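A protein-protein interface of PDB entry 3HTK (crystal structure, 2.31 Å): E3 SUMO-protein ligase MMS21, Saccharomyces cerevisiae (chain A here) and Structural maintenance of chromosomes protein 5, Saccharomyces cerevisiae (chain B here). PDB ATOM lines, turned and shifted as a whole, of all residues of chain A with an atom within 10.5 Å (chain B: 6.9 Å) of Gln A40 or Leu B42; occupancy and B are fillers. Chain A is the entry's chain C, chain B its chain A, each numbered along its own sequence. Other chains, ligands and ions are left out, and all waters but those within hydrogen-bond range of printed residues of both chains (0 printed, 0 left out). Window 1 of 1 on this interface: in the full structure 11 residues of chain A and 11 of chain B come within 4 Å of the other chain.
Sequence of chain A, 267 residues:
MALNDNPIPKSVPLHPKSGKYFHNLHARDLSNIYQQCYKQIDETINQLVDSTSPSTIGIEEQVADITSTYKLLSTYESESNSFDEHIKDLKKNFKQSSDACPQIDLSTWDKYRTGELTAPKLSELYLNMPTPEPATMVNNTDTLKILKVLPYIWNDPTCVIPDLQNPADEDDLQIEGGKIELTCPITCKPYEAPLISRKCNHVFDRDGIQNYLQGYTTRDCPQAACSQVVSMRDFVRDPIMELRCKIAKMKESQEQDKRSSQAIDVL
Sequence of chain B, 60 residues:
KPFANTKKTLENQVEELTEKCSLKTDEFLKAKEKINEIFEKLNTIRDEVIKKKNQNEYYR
The backbone carbonyl oxygen (O) of Phe B39 sits close to the side-chain amide oxygen (OE1) of Gln A40 (3.5 Å). OE1 of Gln A40 lies close to OD1 of Asn B43 (3.0 Å). NH2 of Arg B46 lies within hydrogen-bond range of O of Gln A40 (2.7 Å). NE of Arg B46 sits close to O of Glu A43, at 3.4 Å. The side-chain hydroxyl (OG1) of Thr A44 lies within hydrogen-bond range of the guanidinium group (NH2) of Arg B46 (2.6 Å). The side-chain amide nitrogen of Gln A47 lies within hydrogen-bond range of the backbone carbonyl oxygen of Arg B46 (3.1 Å).
CZ of Phe B39 touches O of Ile A33, at 3.8 Å. Gln A36 touches Phe B39. Cys A37 touches Phe B39 (SG to CZ, 3.8 Å). Leu B42 touches Gln A40 (CB to NE2, 3.0 Å).
O of Phe B39 sits at hydrogen-bond distance from ND2 of Asn B43, at 3.0 Å. The guanidinium group (NH1) of Arg B46 sits at hydrogen-bond distance from the backbone carbonyl oxygen (O) of Leu B42, 2.9 Å away. The backbone carbonyl oxygen of Ile A33 lies within hydrogen-bond range of the side-chain sulfur of Cys A37. O of Gln A40 sits at hydrogen-bond distance from OG1 of Thr A44.
Of the 11 printed residues of chain B, 4 touch a printed residue of chain A. Along chain B the printed residues that touch a printed residue of chain A span positions 39 to 46. Of the 23 printed residues of chain A, 7 touch a printed residue of chain B. Printed residues of chain A that touch a printed residue of chain B: Ile A33, Gln A36, Cys A37, Gln A40, Glu A43, Thr A44 and Gln A47. Among the printed residues, 10 pairs touch across the chains. Among the printed residues, no Asp or Glu carboxylate lies within 4 Å of a Lys or Arg side-chain nitrogen of the other chain.
Gln A40 touches four residues of chain B. Leu B42 touches one residue of chain A. Asn B43 touches just one residue of chain A: Gln A40 (3.0 Å). No residue of chain A comes within 4 Å of Thr B44. Arg B46 touches just these residues of chain A: Gln A40, Glu A43, Thr A44 and Gln A47. Printed residues of chain B within 4 Å of Thr A44: Arg B46 (2.6 Å). Of the printed residues of chain B, Gln A47 touches Arg B46 (3.1 Å). Of the printed residues of chain B, Cys A37 touches Phe B39. Leu A147 touches none of the printed residues of chain B. Lys B41 touches none of the printed residues of chain A. The nearest residue of chain B that does not touch Gln A40 is Glu B40 (5.3 Å). The nearest residue of chain A that does not touch Leu B42 is Thr A44 (5.0 Å). The nearest printed residue of chain B that does not touch Gln A47 is Ile B45 (4.9 Å).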
ATOM      1  N   ASN A  32      -2.995  15.763  26.340  1.00  0.00           N
ATOM      2  CA  ASN A  32      -3.568  14.543  26.872  1.00  0.00           C
ATOM      3  C   ASN A  32      -3.324  13.345  25.959  1.00  0.00           C
ATOM      4  O   ASN A  32      -3.122  12.224  26.431  1.00  0.00           O
ATOM      5  CB  ASN A  32      -5.071  14.718  27.076  1.00  0.00           C
ATOM      6  CG  ASN A  32      -5.753  13.426  27.456  1.00  0.00           C
ATOM      7  OD1 ASN A  32      -6.930  13.222  27.160  1.00  0.00           O
ATOM      8  ND2 ASN A  32      -5.018  12.543  28.127  1.00  0.00           N
ATOM      9  N   ILE A  33      -3.355  13.577  24.652  1.00  0.00           N
ATOM     10  CA  ILE A  33      -3.149  12.496  23.705  1.00  0.00           C
ATOM     11  C   ILE A  33      -1.681  12.091  23.631  1.00  0.00           C
ATOM     12  O   ILE A  33      -1.361  10.905  23.608  1.00  0.00           O
ATOM     13  CB  ILE A  33      -3.709  12.890  22.317  1.00  0.00           C
ATOM     14  CG1 ILE A  33      -5.228  13.054  22.448  1.00  0.00           C
ATOM     15  CG2 ILE A  33      -3.371  11.826  21.265  1.00  0.00           C
ATOM     16  CD1 ILE A  33      -5.983  13.007  21.141  1.00  0.00           C
ATOM     17  N   TYR A  34      -0.792  13.080  23.611  1.00  0.00           N
ATOM     18  CA  TYR A  34       0.646  12.821  23.577  1.00  0.00           C
ATOM     19  C   TYR A  34       1.030  12.001  24.804  1.00  0.00           C
ATOM     20  O   TYR A  34       1.821  11.059  24.723  1.00  0.00           O
ATOM     21  CB  TYR A  34       1.408  14.141  23.590  1.00  0.00           C
ATOM     22  CG  TYR A  34       1.591  14.765  22.234  1.00  0.00           C
ATOM     23  CD1 TYR A  34       1.204  16.081  21.993  1.00  0.00           C
ATOM     24  CD2 TYR A  34       2.169  14.043  21.187  1.00  0.00           C
ATOM     25  CE1 TYR A  34       1.382  16.664  20.742  1.00  0.00           C
ATOM     26  CE2 TYR A  34       2.353  14.618  19.936  1.00  0.00           C
ATOM     27  CZ  TYR A  34       1.954  15.929  19.722  1.00  0.00           C
ATOM     28  OH  TYR A  34       2.112  16.489  18.480  1.00  0.00           O
ATOM     29  N   GLN A  35       0.447  12.377  25.938  1.00  0.00           N
ATOM     30  CA  GLN A  35       0.681  11.720  27.221  1.00  0.00           C
ATOM     31  C   GLN A  35       0.365  10.236  27.134  1.00  0.00           C
ATOM     32  O   GLN A  35       1.159   9.402  27.577  1.00  0.00           O
ATOM     33  CB  GLN A  35      -0.191  12.385  28.282  1.00  0.00           C
ATOM     34  CG  GLN A  35      -0.210  11.718  29.640  1.00  0.00           C
ATOM     35  CD  GLN A  35      -1.233  12.371  30.564  1.00  0.00           C
ATOM     36  OE1 GLN A  35      -1.250  13.597  30.719  1.00  0.00           O
ATOM     37  NE2 GLN A  35      -2.091  11.556  31.177  1.00  0.00           N
ATOM     38  N   GLN A  36      -0.796   9.914  26.570  1.00  0.00           N
ATOM     39  CA  GLN A  36      -1.219   8.532  26.402  1.00  0.00           C
ATOM     40  C   GLN A  36      -0.327   7.808  25.397  1.00  0.00           C
ATOM     41  O   GLN A  36      -0.098   6.597  25.517  1.00  0.00           O
ATOM     42  CB  GLN A  36      -2.673   8.470  25.919  1.00  0.00           C
ATOM     43  CG  GLN A  36      -3.709   8.811  26.987  1.00  0.00           C
ATOM     44  CD  GLN A  36      -5.135   8.826  26.447  1.00  0.00           C
ATOM     45  OE1 GLN A  36      -5.518   9.722  25.691  1.00  0.00           O
ATOM     46  NE2 GLN A  36      -5.924   7.828  26.829  1.00  0.00           N
ATOM     47  N   CYS A  37       0.159   8.534  24.389  1.00  0.00           N
ATOM     48  CA  CYS A  37       1.032   7.910  23.404  1.00  0.00           C
ATOM     49  C   CYS A  37       2.310   7.465  24.099  1.00  0.00           C
ATOM     50  O   CYS A  37       2.809   6.379  23.852  1.00  0.00           O
ATOM     51  CB  CYS A  37       1.388   8.886  22.267  1.00  0.00           C
ATOM     52  SG  CYS A  37       0.055   9.171  21.067  1.00  0.00           S
ATOM     53  N   TYR A  38       2.846   8.321  24.960  1.00  0.00           N
ATOM     54  CA  TYR A  38       4.070   7.983  25.676  1.00  0.00           C
ATOM     55  C   TYR A  38       3.813   6.845  26.662  1.00  0.00           C
ATOM     56  O   TYR A  38       4.647   5.953  26.816  1.00  0.00           O
ATOM     57  CB  TYR A  38       4.603   9.204  26.407  1.00  0.00           C
ATOM     58  CG  TYR A  38       5.178  10.252  25.483  1.00  0.00           C
ATOM     59  CD1 TYR A  38       6.299   9.975  24.701  1.00  0.00           C
ATOM     60  CD2 TYR A  38       4.630  11.528  25.416  1.00  0.00           C
ATOM     61  CE1 TYR A  38       6.865  10.947  23.886  1.00  0.00           C
ATOM     62  CE2 TYR A  38       5.186  12.501  24.604  1.00  0.00           C
ATOM     63  CZ  TYR A  38       6.305  12.208  23.843  1.00  0.00           C
ATOM     64  OH  TYR A  38       6.876  13.176  23.051  1.00  0.00           O
ATOM     65  N   LYS A  39       2.656   6.871  27.320  1.00  0.00           N
ATOM     66  CA  LYS A  39       2.311   5.815  28.260  1.00  0.00           C
ATOM     67  C   LYS A  39       2.172   4.507  27.504  1.00  0.00           C
ATOM     68  O   LYS A  39       2.621   3.462  27.984  1.00  0.00           O
ATOM     69  CB  LYS A  39       1.010   6.135  28.998  1.00  0.00           C
ATOM     70  CG  LYS A  39       1.139   7.306  29.952  1.00  0.00           C
ATOM     71  CD  LYS A  39      -0.153   7.549  30.701  1.00  0.00           C
ATOM     72  CE  LYS A  39       0.032   8.568  31.822  1.00  0.00           C
ATOM     73  NZ  LYS A  39      -1.245   8.783  32.569  1.00  0.00           N
ATOM     74  N   GLN A  40       1.553   4.557  26.325  1.00  0.00           N
ATOM     75  CA  GLN A  40       1.395   3.352  25.525  1.00  0.00           C
ATOM     76  C   GLN A  40       2.798   2.840  25.167  1.00  0.00           C
ATOM     77  O   GLN A  40       3.067   1.634  25.207  1.00  0.00           O
ATOM     78  CB  GLN A  40       0.579   3.652  24.264  1.00  0.00           C
ATOM     79  CG  GLN A  40      -0.921   3.846  24.528  1.00  0.00           C
ATOM     80  CD  GLN A  40      -1.647   2.547  24.902  1.00  0.00           C
ATOM     81  OE1 GLN A  40      -2.731   2.571  25.492  1.00  0.00           O
ATOM     82  NE2 GLN A  40      -1.057   1.415  24.544  1.00  0.00           N
ATOM     83  N   ILE A  41       3.690   3.765  24.827  1.00  0.00           N
ATOM     84  CA  ILE A  41       5.071   3.410  24.505  1.00  0.00           C
ATOM     85  C   ILE A  41       5.710   2.662  25.700  1.00  0.00           C
ATOM     86  O   ILE A  41       6.252   1.561  25.552  1.00  0.00           O
ATOM     87  CB  ILE A  41       5.930   4.672  24.226  1.00  0.00           C
ATOM     88  CG1 ILE A  41       5.502   5.338  22.909  1.00  0.00           C
ATOM     89  CG2 ILE A  41       7.408   4.285  24.176  1.00  0.00           C
ATOM     90  CD1 ILE A  41       5.883   4.555  21.675  1.00  0.00           C
ATOM     91  N   ASP A  42       5.645   3.275  26.881  1.00  0.00           N
ATOM     92  CA  ASP A  42       6.215   2.671  28.079  1.00  0.00           C
ATOM     93  C   ASP A  42       5.727   1.253  28.319  1.00  0.00           C
ATOM     94  O   ASP A  42       6.522   0.316  28.374  1.00  0.00           O
ATOM     95  CB  ASP A  42       5.918   3.527  29.307  1.00  0.00           C
ATOM     96  CG  ASP A  42       6.881   4.679  29.449  1.00  0.00           C
ATOM     97  OD1 ASP A  42       7.958   4.639  28.807  1.00  0.00           O
ATOM     98  OD2 ASP A  42       6.571   5.617  30.214  1.00  0.00           O
ATOM     99  N   GLU A  43       4.417   1.103  28.456  1.00  0.00           N
ATOM    100  CA  GLU A  43       3.817  -0.200  28.681  1.00  0.00           C
ATOM    101  C   GLU A  43       4.245  -1.246  27.664  1.00  0.00           C
ATOM    102  O   GLU A  43       4.050  -2.443  27.884  1.00  0.00           O
ATOM    103  CB  GLU A  43       2.290  -0.073  28.694  1.00  0.00           C
ATOM    104  CG  GLU A  43       1.743   0.472  30.006  1.00  0.00           C
ATOM    105  CD  GLU A  43       2.032  -0.456  31.188  1.00  0.00           C
ATOM    106  OE1 GLU A  43       1.862  -0.017  32.348  1.00  0.00           O
ATOM    107  OE2 GLU A  43       2.423  -1.628  30.959  1.00  0.00           O
ATOM    108  N   THR A  44       4.826  -0.807  26.551  1.00  0.00           N
ATOM    109  CA  THR A  44       5.265  -1.743  25.523  1.00  0.00           C
ATOM    110  C   THR A  44       6.667  -2.266  25.815  1.00  0.00           C
ATOM    111  O   THR A  44       6.967  -3.427  25.525  1.00  0.00           O
ATOM    112  CB  THR A  44       5.229  -1.101  24.122  1.00  0.00           C
ATOM    113  OG1 THR A  44       3.866  -0.874  23.744  1.00  0.00           O
ATOM    114  CG2 THR A  44       5.889  -2.006  23.088  1.00  0.00           C
ATOM    115  N   ILE A  45       7.529  -1.430  26.387  1.00  0.00           N
ATOM    116  CA  ILE A  45       8.869  -1.894  26.708  1.00  0.00           C
ATOM    117  C   ILE A  45       8.748  -2.840  27.907  1.00  0.00           C
ATOM    118  O   ILE A  45       9.442  -3.856  27.985  1.00  0.00           O
ATOM    119  CB  ILE A  45       9.834  -0.732  27.059  1.00  0.00           C
ATOM    120  CG1 ILE A  45       9.587  -0.251  28.486  1.00  0.00           C
ATOM    121  CG2 ILE A  45       9.641   0.432  26.079  1.00  0.00           C
ATOM    122  CD1 ILE A  45      10.599   0.785  28.964  1.00  0.00           C
ATOM    123  N   ASN A  46       7.840  -2.525  28.828  1.00  0.00           N
ATOM    124  CA  ASN A  46       7.659  -3.374  29.996  1.00  0.00           C
ATOM    125  C   ASN A  46       7.324  -4.789  29.552  1.00  0.00           C
ATOM    126  O   ASN A  46       8.065  -5.720  29.854  1.00  0.00           O
ATOM    127  CB  ASN A  46       6.564  -2.826  30.909  1.00  0.00           C
ATOM    128  CG  ASN A  46       6.890  -1.440  31.438  1.00  0.00           C
ATOM    129  OD1 ASN A  46       8.046  -1.131  31.738  1.00  0.00           O
ATOM    130  ND2 ASN A  46       5.869  -0.596  31.561  1.00  0.00           N
ATOM    131  N   GLN A  47       6.227  -4.957  28.820  1.00  0.00           N
ATOM    132  CA  GLN A  47       5.854  -6.285  28.355  1.00  0.00           C
ATOM    133  C   GLN A  47       6.917  -6.903  27.464  1.00  0.00           C
ATOM    134  O   GLN A  47       7.053  -8.126  27.394  1.00  0.00           O
ATOM    135  CB  GLN A  47       4.546  -6.244  27.577  1.00  0.00           C
ATOM    136  CG  GLN A  47       3.339  -5.899  28.403  1.00  0.00           C
ATOM    137  CD  GLN A  47       2.124  -6.696  27.970  1.00  0.00           C
ATOM    138  OE1 GLN A  47       1.993  -7.066  26.800  1.00  0.00           O
ATOM    139  NE2 GLN A  47       1.226  -6.963  28.909  1.00  0.00           N
ATOM    140  N   LEU A  48       7.650  -6.053  26.755  1.00  0.00           N
ATOM    141  CA  LEU A  48       8.707  -6.519  25.872  1.00  0.00           C
ATOM    142  C   LEU A  48       9.779  -7.162  26.748  1.00  0.00           C
ATOM    143  O   LEU A  48      10.134  -8.317  26.563  1.00  0.00           O
ATOM    144  CB  LEU A  48       9.288  -5.339  25.088  1.00  0.00           C
ATOM    145  CG  LEU A  48      10.179  -5.603  23.870  1.00  0.00           C
ATOM    146  CD1 LEU A  48      11.531  -6.136  24.312  1.00  0.00           C
ATOM    147  CD2 LEU A  48       9.489  -6.572  22.924  1.00  0.00           C
ATOM    148  N   ILE A  66      10.897   0.502  18.344  1.00  0.00           N
ATOM    149  CA  ILE A  66      10.264   1.316  19.366  1.00  0.00           C
ATOM    150  C   ILE A  66      10.878   2.706  19.452  1.00  0.00           C
ATOM    151  O   ILE A  66      10.163   3.695  19.548  1.00  0.00           O
ATOM    152  CB  ILE A  66      10.363   0.624  20.748  1.00  0.00           C
ATOM    153  CG1 ILE A  66       9.584  -0.690  20.720  1.00  0.00           C
ATOM    154  CG2 ILE A  66       9.828   1.526  21.840  1.00  0.00           C
ATOM    155  CD1 ILE A  66       8.140  -0.533  20.381  1.00  0.00           C
ATOM    156  N   THR A  69       9.671   5.014  16.616  1.00  0.00           N
ATOM    157  CA  THR A  69       8.382   5.685  16.748  1.00  0.00           C
ATOM    158  C   THR A  69       8.426   6.641  17.930  1.00  0.00           C
ATOM    159  O   THR A  69       7.799   7.691  17.907  1.00  0.00           O
ATOM    160  CB  THR A  69       7.187   4.703  16.941  1.00  0.00           C
ATOM    161  OG1 THR A  69       7.073   4.342  18.319  1.00  0.00           O
ATOM    162  CG2 THR A  69       7.361   3.469  16.098  1.00  0.00           C
ATOM    163  N   TYR A  70       9.172   6.288  18.967  1.00  0.00           N
ATOM    164  CA  TYR A  70       9.266   7.177  20.109  1.00  0.00           C
ATOM    165  C   TYR A  70       9.803   8.532  19.658  1.00  0.00           C
ATOM    166  O   TYR A  70       9.253   9.573  20.010  1.00  0.00           O
ATOM    167  CB  TYR A  70      10.199   6.622  21.168  1.00  0.00           C
ATOM    168  CG  TYR A  70      10.381   7.576  22.324  1.00  0.00           C
ATOM    169  CD1 TYR A  70       9.403   7.694  23.303  1.00  0.00           C
ATOM    170  CD2 TYR A  70      11.517   8.384  22.424  1.00  0.00           C
ATOM    171  CE1 TYR A  70       9.539   8.580  24.350  1.00  0.00           C
ATOM    172  CE2 TYR A  70      11.664   9.288  23.483  1.00  0.00           C
ATOM    173  CZ  TYR A  70      10.664   9.373  24.439  1.00  0.00           C
ATOM    174  OH  TYR A  70      10.769  10.248  25.497  1.00  0.00           O
ATOM    175  N   LEU A  73       7.135  10.450  17.509  1.00  0.00           N
ATOM    176  CA  LEU A  73       6.167  11.065  18.402  1.00  0.00           C
ATOM    177  C   LEU A  73       6.762  12.297  19.062  1.00  0.00           C
ATOM    178  O   LEU A  73       6.107  13.338  19.145  1.00  0.00           O
ATOM    179  CB  LEU A  73       5.754  10.081  19.487  1.00  0.00           C
ATOM    180  CG  LEU A  73       4.512  10.497  20.266  1.00  0.00           C
ATOM    181  CD1 LEU A  73       3.268   9.988  19.535  1.00  0.00           C
ATOM    182  CD2 LEU A  73       4.577   9.918  21.666  1.00  0.00           C
ATOM    183  N   THR A 143      12.385   7.674  29.558  1.00  0.00           N
ATOM    184  CA  THR A 143      12.053   6.566  28.665  1.00  0.00           C
ATOM    185  C   THR A 143      13.026   6.398  27.495  1.00  0.00           C
ATOM    186  O   THR A 143      13.091   5.330  26.883  1.00  0.00           O
ATOM    187  CB  THR A 143      10.590   6.695  28.142  1.00  0.00           C
ATOM    188  OG1 THR A 143      10.450   5.989  26.902  1.00  0.00           O
ATOM    189  CG2 THR A 143      10.201   8.155  27.964  1.00  0.00           C
ATOM    190  N   LEU A 147      15.644   2.915  26.604  1.00  0.00           N
ATOM    191  CA  LEU A 147      15.740   2.363  25.255  1.00  0.00           C
ATOM    192  C   LEU A 147      17.196   2.257  24.827  1.00  0.00           C
ATOM    193  O   LEU A 147      17.623   1.237  24.288  1.00  0.00           O
ATOM    194  CB  LEU A 147      14.980   3.239  24.262  1.00  0.00           C
ATOM    195  CG  LEU A 147      13.450   3.213  24.343  1.00  0.00           C
ATOM    196  CD1 LEU A 147      12.870   4.283  23.428  1.00  0.00           C
ATOM    197  CD2 LEU A 147      12.943   1.831  23.949  1.00  0.00           C
ATOM    198  N   GLU B  37      -8.989   4.577  19.274  1.00  0.00           N
ATOM    199  CA  GLU B  37      -9.294   3.189  18.951  1.00  0.00           C
ATOM    200  C   GLU B  37      -7.987   2.398  19.004  1.00  0.00           C
ATOM    201  O   GLU B  37      -7.976   1.213  19.346  1.00  0.00           O
ATOM    202  CB  GLU B  37      -9.884   3.060  17.552  1.00  0.00           C
ATOM    203  CG  GLU B  37     -11.270   3.626  17.363  1.00  0.00           C
ATOM    204  CD  GLU B  37     -11.699   3.566  15.904  1.00  0.00           C
ATOM    205  OE1 GLU B  37     -11.667   2.459  15.328  1.00  0.00           O
ATOM    206  OE2 GLU B  37     -12.060   4.620  15.332  1.00  0.00           O
ATOM    207  N   ILE B  38      -6.885   3.058  18.652  1.00  0.00           N
ATOM    208  CA  ILE B  38      -5.583   2.416  18.665  1.00  0.00           C
ATOM    209  C   ILE B  38      -5.089   2.234  20.116  1.00  0.00           C
ATOM    210  O   ILE B  38      -4.482   1.218  20.445  1.00  0.00           O
ATOM    211  CB  ILE B  38      -4.566   3.215  17.800  1.00  0.00           C
ATOM    212  CG1 ILE B  38      -4.964   3.100  16.321  1.00  0.00           C
ATOM    213  CG2 ILE B  38      -3.170   2.655  17.965  1.00  0.00           C
ATOM    214  CD1 ILE B  38      -4.280   4.110  15.405  1.00  0.00           C
ATOM    215  N   PHE B  39      -5.352   3.204  20.984  1.00  0.00           N
ATOM    216  CA  PHE B  39      -4.970   3.047  22.382  1.00  0.00           C
ATOM    217  C   PHE B  39      -5.732   1.806  22.878  1.00  0.00           C
ATOM    218  O   PHE B  39      -5.218   0.991  23.651  1.00  0.00           O
ATOM    219  CB  PHE B  39      -5.426   4.251  23.200  1.00  0.00           C
ATOM    220  CG  PHE B  39      -4.696   5.519  22.880  1.00  0.00           C
ATOM    221  CD1 PHE B  39      -5.290   6.754  23.121  1.00  0.00           C
ATOM    222  CD2 PHE B  39      -3.395   5.484  22.367  1.00  0.00           C
ATOM    223  CE1 PHE B  39      -4.603   7.937  22.857  1.00  0.00           C
ATOM    224  CE2 PHE B  39      -2.706   6.653  22.107  1.00  0.00           C
ATOM    225  CZ  PHE B  39      -3.309   7.886  22.350  1.00  0.00           C
ATOM    226  N   GLU B  40      -6.972   1.675  22.416  1.00  0.00           N
ATOM    227  CA  GLU B  40      -7.809   0.562  22.822  1.00  0.00           C
ATOM    228  C   GLU B  40      -7.292  -0.786  22.348  1.00  0.00           C
ATOM    229  O   GLU B  40      -7.273  -1.731  23.123  1.00  0.00           O
ATOM    230  CB  GLU B  40      -9.244   0.762  22.336  1.00  0.00           C
ATOM    231  CG  GLU B  40     -10.247   0.714  23.461  1.00  0.00           C
ATOM    232  CD  GLU B  40      -9.969   1.775  24.517  1.00  0.00           C
ATOM    233  OE1 GLU B  40     -10.113   2.980  24.208  1.00  0.00           O
ATOM    234  OE2 GLU B  40      -9.599   1.400  25.653  1.00  0.00           O
ATOM    235  N   LYS B  41      -6.892  -0.883  21.084  1.00  0.00           N
ATOM    236  CA  LYS B  41      -6.374  -2.142  20.561  1.00  0.00           C
ATOM    237  C   LYS B  41      -5.072  -2.504  21.267  1.00  0.00           C
ATOM    238  O   LYS B  41      -4.828  -3.675  21.559  1.00  0.00           O
ATOM    239  CB  LYS B  41      -6.163  -2.054  19.048  1.00  0.00           C
ATOM    240  CG  LYS B  41      -7.474  -1.953  18.267  1.00  0.00           C
ATOM    241  CD  LYS B  41      -7.256  -1.911  16.751  1.00  0.00           C
ATOM    242  CE  LYS B  41      -8.544  -1.517  16.014  1.00  0.00           C
ATOM    243  NZ  LYS B  41      -8.368  -1.420  14.529  1.00  0.00           N
ATOM    244  N   LEU B  42      -4.240  -1.502  21.547  1.00  0.00           N
ATOM    245  CA  LEU B  42      -2.985  -1.731  22.258  1.00  0.00           C
ATOM    246  C   LEU B  42      -3.280  -2.303  23.655  1.00  0.00           C
ATOM    247  O   LEU B  42      -2.654  -3.278  24.082  1.00  0.00           O
ATOM    248  CB  LEU B  42      -2.180  -0.418  22.383  1.00  0.00           C
ATOM    249  CG  LEU B  42      -1.393   0.087  21.157  1.00  0.00           C
ATOM    250  CD1 LEU B  42      -0.836   1.482  21.424  1.00  0.00           C
ATOM    251  CD2 LEU B  42      -0.252  -0.864  20.842  1.00  0.00           C
ATOM    252  N   ASN B  43      -4.242  -1.700  24.354  1.00  0.00           N
ATOM    253  CA  ASN B  43      -4.619  -2.136  25.697  1.00  0.00           C
ATOM    254  C   ASN B  43      -5.125  -3.571  25.763  1.00  0.00           C
ATOM    255  O   ASN B  43      -4.735  -4.337  26.643  1.00  0.00           O
ATOM    256  CB  ASN B  43      -5.705  -1.233  26.274  1.00  0.00           C
ATOM    257  CG  ASN B  43      -5.204   0.149  26.613  1.00  0.00           C
ATOM    258  OD1 ASN B  43      -4.034   0.340  26.969  1.00  0.00           O
ATOM    259  ND2 ASN B  43      -6.102   1.128  26.533  1.00  0.00           N
ATOM    260  N   THR B  44      -6.014  -3.931  24.851  1.00  0.00           N
ATOM    261  CA  THR B  44      -6.552  -5.279  24.866  1.00  0.00           C
ATOM    262  C   THR B  44      -5.444  -6.288  24.571  1.00  0.00           C
ATOM    263  O   THR B  44      -5.330  -7.300  25.269  1.00  0.00           O
ATOM    264  CB  THR B  44      -7.743  -5.438  23.862  1.00  0.00           C
ATOM    265  OG1 THR B  44      -7.279  -5.293  22.517  1.00  0.00           O
ATOM    266  CG2 THR B  44      -8.802  -4.374  24.128  1.00  0.00           C
ATOM    267  N   ILE B  45      -4.621  -6.025  23.553  1.00  0.00           N
ATOM    268  CA  ILE B  45      -3.525  -6.941  23.240  1.00  0.00           C
ATOM    269  C   ILE B  45      -2.683  -7.197  24.502  1.00  0.00           C
ATOM    270  O   ILE B  45      -2.315  -8.336  24.784  1.00  0.00           O
ATOM    271  CB  ILE B  45      -2.590  -6.392  22.120  1.00  0.00           C
ATOM    272  CG1 ILE B  45      -3.085  -6.825  20.730  1.00  0.00           C
ATOM    273  CG2 ILE B  45      -1.196  -6.959  22.284  1.00  0.00           C
ATOM    274  CD1 ILE B  45      -4.451  -6.326  20.355  1.00  0.00           C
ATOM    275  N   ARG B  46      -2.381  -6.139  25.255  1.00  0.00           N
ATOM    276  CA  ARG B  46      -1.585  -6.286  26.466  1.00  0.00           C
ATOM    277  C   ARG B  46      -2.253  -7.235  27.456  1.00  0.00           C
ATOM    278  O   ARG B  46      -1.579  -8.012  28.135  1.00  0.00           O
ATOM    279  CB  ARG B  46      -1.353  -4.932  27.136  1.00  0.00           C
ATOM    280  CG  ARG B  46      -0.245  -4.106  26.493  1.00  0.00           C
ATOM    281  CD  ARG B  46       0.027  -2.839  27.291  1.00  0.00           C
ATOM    282  NE  ARG B  46       0.934  -1.933  26.589  1.00  0.00           N
ATOM    283  CZ  ARG B  46       0.642  -1.310  25.450  1.00  0.00           C
ATOM    284  NH1 ARG B  46      -0.537  -1.484  24.874  1.00  0.00           N
ATOM    285  NH2 ARG B  46       1.531  -0.509  24.883  1.00  0.00           N
ATOM    286  N   ASP B  47      -3.580  -7.162  27.535  1.00  0.00           N
ATOM    287  CA  ASP B  47      -4.329  -8.025  28.430  1.00  0.00           C
ATOM    288  C   ASP B  47      -4.151  -9.466  28.008  1.00  0.00           C
ATOM    289  O   ASP B  47      -4.020 -10.347  28.853  1.00  0.00           O
ATOM    290  CB  ASP B  47      -5.810  -7.662  28.429  1.00  0.00           C
ATOM    291  CG  ASP B  47      -6.093  -6.396  29.201  1.00  0.00           C
ATOM    292  OD1 ASP B  47      -5.547  -6.247  30.321  1.00  0.00           O
ATOM    293  OD2 ASP B  47      -6.868  -5.555  28.690  1.00  0.00           O
